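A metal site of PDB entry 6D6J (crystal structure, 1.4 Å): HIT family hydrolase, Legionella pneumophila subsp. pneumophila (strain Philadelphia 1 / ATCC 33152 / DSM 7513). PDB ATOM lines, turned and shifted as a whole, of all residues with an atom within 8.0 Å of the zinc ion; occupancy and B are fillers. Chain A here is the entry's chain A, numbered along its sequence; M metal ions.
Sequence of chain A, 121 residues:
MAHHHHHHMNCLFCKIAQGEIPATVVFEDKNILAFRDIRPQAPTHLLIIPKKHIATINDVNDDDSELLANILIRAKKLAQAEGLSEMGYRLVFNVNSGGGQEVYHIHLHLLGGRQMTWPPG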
ATOM      1  N   ASN A  10      39.153 -14.656 -11.976  1.00  0.00           N
ATOM      2  CA  ASN A  10      39.145 -13.718 -13.084  1.00  0.00           C
ATOM      3  C   ASN A  10      37.745 -13.139 -13.341  1.00  0.00           C
ATOM      4  O   ASN A  10      37.492 -12.567 -14.401  1.00  0.00           O
ATOM      5  CB  ASN A  10      39.641 -14.408 -14.357  1.00  0.00           C
ATOM      6  N   CYS A  11      36.844 -13.268 -12.377  1.00  0.00           N
ATOM      7  CA  CYS A  11      35.463 -12.865 -12.557  1.00  0.00           C
ATOM      8  C   CYS A  11      35.244 -11.496 -11.921  1.00  0.00           C
ATOM      9  O   CYS A  11      35.463 -11.321 -10.717  1.00  0.00           O
ATOM     10  CB  CYS A  11      34.530 -13.896 -11.933  1.00  0.00           C
ATOM     11  SG  CYS A  11      32.798 -13.357 -11.980  1.00  0.00           S
ATOM     12  N   LEU A  12      34.799 -10.540 -12.730  1.00  0.00           N
ATOM     13  CA  LEU A  12      34.566  -9.178 -12.250  1.00  0.00           C
ATOM     14  C   LEU A  12      33.602  -9.151 -11.082  1.00  0.00           C
ATOM     15  O   LEU A  12      33.808  -8.422 -10.101  1.00  0.00           O
ATOM     16  CB  LEU A  12      34.054  -8.304 -13.396  1.00  0.00           C
ATOM     17  CG  LEU A  12      33.570  -6.899 -13.028  1.00  0.00           C
ATOM     18  CD1 LEU A  12      34.687  -6.071 -12.418  1.00  0.00           C
ATOM     19  CD2 LEU A  12      32.966  -6.201 -14.244  1.00  0.00           C
ATOM     20  N   PHE A  13      32.512  -9.915 -11.177  1.00  0.00           N
ATOM     21  CA  PHE A  13      31.487  -9.869 -10.143  1.00  0.00           C
ATOM     22  C   PHE A  13      31.904 -10.617  -8.882  1.00  0.00           C
ATOM     23  O   PHE A  13      31.512 -10.214  -7.775  1.00  0.00           O
ATOM     24  CB  PHE A  13      30.135 -10.325 -10.681  1.00  0.00           C
ATOM     25  CG  PHE A  13      29.486  -9.335 -11.641  1.00  0.00           C
ATOM     26  CD1 PHE A  13      30.050  -8.079 -11.881  1.00  0.00           C
ATOM     27  CD2 PHE A  13      28.309  -9.658 -12.297  1.00  0.00           C
ATOM     28  CE1 PHE A  13      29.447  -7.165 -12.767  1.00  0.00           C
ATOM     29  CE2 PHE A  13      27.715  -8.762 -13.173  1.00  0.00           C
ATOM     30  CZ  PHE A  13      28.268  -7.514 -13.408  1.00  0.00           C
ATOM     31  N   CYS A  14      32.720 -11.674  -9.010  1.00  0.00           N
ATOM     32  CA  CYS A  14      33.329 -12.265  -7.816  1.00  0.00           C
ATOM     33  C   CYS A  14      34.218 -11.254  -7.119  1.00  0.00           C
ATOM     34  O   CYS A  14      34.207 -11.154  -5.876  1.00  0.00           O
ATOM     35  CB  CYS A  14      34.108 -13.529  -8.161  1.00  0.00           C
ATOM     36  SG  CYS A  14      33.039 -14.970  -8.432  1.00  0.00           S
ATOM     37  N   LYS A  15      35.010 -10.494  -7.883  1.00  0.00           N
ATOM     38  CA  LYS A  15      35.876  -9.498  -7.256  1.00  0.00           C
ATOM     39  C   LYS A  15      35.057  -8.430  -6.539  1.00  0.00           C
ATOM     40  O   LYS A  15      35.412  -8.019  -5.432  1.00  0.00           O
ATOM     41  CB  LYS A  15      36.773  -8.845  -8.312  1.00  0.00           C
ATOM     42  CG  LYS A  15      37.852  -9.740  -8.895  1.00  0.00           C
ATOM     43  CD  LYS A  15      38.638  -8.938  -9.932  1.00  0.00           C
ATOM     44  CE  LYS A  15      39.556  -9.753 -10.793  1.00  0.00           C
ATOM     45  NZ  LYS A  15      39.942  -8.920 -11.975  1.00  0.00           N
ATOM     46  N   ILE A  16      33.935  -8.012  -7.133  1.00  0.00           N
ATOM     47  CA  ILE A  16      33.078  -7.035  -6.477  1.00  0.00           C
ATOM     48  C   ILE A  16      32.439  -7.643  -5.233  1.00  0.00           C
ATOM     49  O   ILE A  16      32.420  -7.027  -4.165  1.00  0.00           O
ATOM     50  CB  ILE A  16      32.022  -6.497  -7.464  1.00  0.00           C
ATOM     51  CG1 ILE A  16      32.713  -5.650  -8.547  1.00  0.00           C
ATOM     52  CG2 ILE A  16      30.956  -5.702  -6.739  1.00  0.00           C
ATOM     53  CD1 ILE A  16      31.794  -5.174  -9.661  1.00  0.00           C
ATOM     54  N   ALA A  17      31.941  -8.875  -5.361  1.00  0.00           N
ATOM     55  CA  ALA A  17      31.315  -9.549  -4.231  1.00  0.00           C
ATOM     56  C   ALA A  17      32.249  -9.635  -3.033  1.00  0.00           C
ATOM     57  O   ALA A  17      31.808  -9.539  -1.878  1.00  0.00           O
ATOM     58  CB  ALA A  17      30.877 -10.956  -4.655  1.00  0.00           C
ATOM     59  N   ILE A  49      23.413  -9.556  -7.376  1.00  0.00           N
ATOM     60  CA  ILE A  49      24.211 -10.744  -7.701  1.00  0.00           C
ATOM     61  C   ILE A  49      24.251 -11.685  -6.512  1.00  0.00           C
ATOM     62  O   ILE A  49      24.292 -11.243  -5.360  1.00  0.00           O
ATOM     63  CB  ILE A  49      25.641 -10.406  -8.162  1.00  0.00           C
ATOM     64  CG1 ILE A  49      26.472  -9.752  -7.049  1.00  0.00           C
ATOM     65  CG2 ILE A  49      25.600  -9.544  -9.394  1.00  0.00           C
ATOM     66  CD1 ILE A  49      27.964  -9.677  -7.399  1.00  0.00           C
ATOM     67  N   PRO A  50      24.284 -12.985  -6.748  1.00  0.00           N
ATOM     68  CA  PRO A  50      24.718 -13.891  -5.691  1.00  0.00           C
ATOM     69  C   PRO A  50      26.211 -13.720  -5.473  1.00  0.00           C
ATOM     70  O   PRO A  50      26.958 -13.416  -6.404  1.00  0.00           O
ATOM     71  CB  PRO A  50      24.419 -15.273  -6.278  1.00  0.00           C
ATOM     72  CG  PRO A  50      24.597 -15.080  -7.757  1.00  0.00           C
ATOM     73  CD  PRO A  50      24.179 -13.660  -8.059  1.00  0.00           C
ATOM     74  N   LYS A  51      26.651 -13.905  -4.235  1.00  0.00           N
ATOM     75  CA  LYS A  51      28.085 -14.017  -4.005  1.00  0.00           C
ATOM     76  C   LYS A  51      28.635 -15.314  -4.593  1.00  0.00           C
ATOM     77  O   LYS A  51      29.757 -15.315  -5.117  1.00  0.00           O
ATOM     78  CB  LYS A  51      28.401 -13.837  -2.522  1.00  0.00           C
ATOM     79  CG  LYS A  51      28.143 -12.403  -2.059  1.00  0.00           C
ATOM     80  CD  LYS A  51      28.611 -12.176  -0.635  1.00  0.00           C
ATOM     81  CE  LYS A  51      28.538 -10.698  -0.271  1.00  0.00           C
ATOM     82  NZ  LYS A  51      28.897 -10.454   1.150  1.00  0.00           N
ATOM     83  N   LYS A  52      27.829 -16.381  -4.595  1.00  0.00           N
ATOM     84  CA  LYS A  52      28.197 -17.629  -5.264  1.00  0.00           C
ATOM     85  C   LYS A  52      28.333 -17.398  -6.770  1.00  0.00           C
ATOM     86  O   LYS A  52      27.481 -16.760  -7.386  1.00  0.00           O
ATOM     87  CB  LYS A  52      27.114 -18.678  -4.989  1.00  0.00           C
ATOM     88  CG  LYS A  52      27.330 -20.019  -5.683  1.00  0.00           C
ATOM     89  CD  LYS A  52      26.106 -20.940  -5.556  1.00  0.00           C
ATOM     90  CE  LYS A  52      25.916 -21.418  -4.132  1.00  0.00           C
ATOM     91  NZ  LYS A  52      24.968 -22.554  -4.101  1.00  0.00           N
ATOM     92  N   HIS A  53      29.387 -17.951  -7.363  1.00  0.00           N
ATOM     93  CA  HIS A  53      29.611 -17.827  -8.795  1.00  0.00           C
ATOM     94  C   HIS A  53      28.791 -18.875  -9.560  1.00  0.00           C
ATOM     95  O   HIS A  53      29.083 -20.066  -9.511  1.00  0.00           O
ATOM     96  CB  HIS A  53      31.103 -17.978  -9.104  1.00  0.00           C
ATOM     97  CG  HIS A  53      31.427 -17.848 -10.557  1.00  0.00           C
ATOM     98  ND1 HIS A  53      31.643 -16.615 -11.168  1.00  0.00           N
ATOM     99  CD2 HIS A  53      31.508 -18.778 -11.535  1.00  0.00           C
ATOM    100  CE1 HIS A  53      31.886 -16.811 -12.453  1.00  0.00           C
ATOM    101  NE2 HIS A  53      31.795 -18.108 -12.702  1.00  0.00           N
ATOM    102  N   ILE A  54      27.769 -18.426 -10.271  1.00  0.00           N
ATOM    103  CA  ILE A  54      27.040 -19.220 -11.254  1.00  0.00           C
ATOM    104  C   ILE A  54      27.185 -18.444 -12.568  1.00  0.00           C
ATOM    105  O   ILE A  54      26.874 -17.246 -12.608  1.00  0.00           O
ATOM    106  CB  ILE A  54      25.561 -19.398 -10.880  1.00  0.00           C
ATOM    107  CG1 ILE A  54      25.427 -20.118  -9.537  1.00  0.00           C
ATOM    108  CG2 ILE A  54      24.817 -20.139 -11.988  1.00  0.00           C
ATOM    109  CD1 ILE A  54      24.034 -20.062  -8.961  1.00  0.00           C
ATOM    110  N   ALA A  55      27.704 -19.092 -13.617  1.00  0.00           N
ATOM    111  CA  ALA A  55      28.150 -18.354 -14.802  1.00  0.00           C
ATOM    112  C   ALA A  55      26.975 -17.768 -15.593  1.00  0.00           C
ATOM    113  O   ALA A  55      27.061 -16.650 -16.103  1.00  0.00           O
ATOM    114  CB  ALA A  55      29.008 -19.243 -15.705  1.00  0.00           C
ATOM    115  N   VAL A 103      28.994 -10.355 -18.782  1.00  0.00           N
ATOM    116  CA  VAL A 103      29.754 -10.835 -17.632  1.00  0.00           C
ATOM    117  C   VAL A 103      29.141 -12.158 -17.227  1.00  0.00           C
ATOM    118  O   VAL A 103      27.939 -12.227 -16.935  1.00  0.00           O
ATOM    119  CB  VAL A 103      29.703  -9.833 -16.466  1.00  0.00           C
ATOM    120  CG1 VAL A 103      30.483 -10.373 -15.252  1.00  0.00           C
ATOM    121  CG2 VAL A 103      30.255  -8.466 -16.888  1.00  0.00           C
ATOM    122  N   TYR A 104      29.959 -13.208 -17.170  1.00  0.00           N
ATOM    123  CA  TYR A 104      29.484 -14.572 -16.894  1.00  0.00           C
ATOM    124  C   TYR A 104      29.498 -14.900 -15.408  1.00  0.00           C
ATOM    125  O   TYR A 104      30.181 -15.793 -14.905  1.00  0.00           O
ATOM    126  CB  TYR A 104      30.202 -15.589 -17.795  1.00  0.00           C
ATOM    127  CG  TYR A 104      29.566 -15.482 -19.163  1.00  0.00           C
ATOM    128  CD1 TYR A 104      28.388 -16.173 -19.421  1.00  0.00           C
ATOM    129  CD2 TYR A 104      30.035 -14.608 -20.136  1.00  0.00           C
ATOM    130  CE1 TYR A 104      27.721 -16.037 -20.635  1.00  0.00           C
ATOM    131  CE2 TYR A 104      29.378 -14.463 -21.355  1.00  0.00           C
ATOM    132  CZ  TYR A 104      28.211 -15.189 -21.586  1.00  0.00           C
ATOM    133  OH  TYR A 104      27.526 -15.086 -22.772  1.00  0.00           O
ATOM    134  N   HIS A 105      28.698 -14.115 -14.680  1.00  0.00           N
ATOM    135  CA  HIS A 105      28.307 -14.365 -13.296  1.00  0.00           C
ATOM    136  C   HIS A 105      26.900 -13.799 -13.241  1.00  0.00           C
ATOM    137  O   HIS A 105      26.709 -12.633 -13.583  1.00  0.00           O
ATOM    138  CB  HIS A 105      29.256 -13.601 -12.373  1.00  0.00           C
ATOM    139  CG  HIS A 105      28.988 -13.748 -10.910  1.00  0.00           C
ATOM    140  ND1 HIS A 105      29.965 -14.101 -10.012  1.00  0.00           N
ATOM    141  CD2 HIS A 105      27.871 -13.487 -10.177  1.00  0.00           C
ATOM    142  CE1 HIS A 105      29.466 -14.087  -8.791  1.00  0.00           C
ATOM    143  NE2 HIS A 105      28.198 -13.723  -8.857  1.00  0.00           N
ATOM    144  N   ILE A 106      25.918 -14.610 -12.843  1.00  0.00           N
ATOM    145  CA  ILE A 106      24.525 -14.180 -13.023  1.00  0.00           C
ATOM    146  C   ILE A 106      24.239 -12.897 -12.249  1.00  0.00           C
ATOM    147  O   ILE A 106      24.792 -12.650 -11.165  1.00  0.00           O
ATOM    148  CB  ILE A 106      23.497 -15.280 -12.695  1.00  0.00           C
ATOM    149  CG1 ILE A 106      23.563 -15.698 -11.219  1.00  0.00           C
ATOM    150  CG2 ILE A 106      23.646 -16.455 -13.637  1.00  0.00           C
ATOM    151  CD1 ILE A 106      22.412 -16.577 -10.824  1.00  0.00           C
HETATM  152 ZN    ZN M   1      31.903 -14.715 -10.375  1.00  0.00          ZN
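The zinc ion is bound by a ring nitrogen (ND1) of His 105 (2.1 Å), a ring nitrogen (ND1) of His 53 (2.1 Å), the side-chain sulfur (SG) of Cys 14 (2.3 Å) and the side-chain sulfur (SG) of Cys 11 (2.3 Å).
Of the 19 residues printed, 4 come within 4 Å of the zinc ion.
The nearest printed residue that does not touch the zinc ion is Phe 13 (4.4 Å).
The backbone NH (N) of His 105 lies within hydrogen-bond range of the backbone carbonyl oxygen (O) of Ala 55 (3.3 Å).
A ring nitrogen (NE2) of His 105 lies within hydrogen-bond range of the backbone carbonyl oxygen (O) of Lys 52 (3.4 Å).
A ring nitrogen (NE2) of His 105 sits at hydrogen-bond distance from the backbone carbonyl oxygen (O) of Pro 50 (2.8 Å).
The side-chain sulfur (SG) of Cys 11 lies close to the backbone NH (N) of Phe 13, 3.5 Å away.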
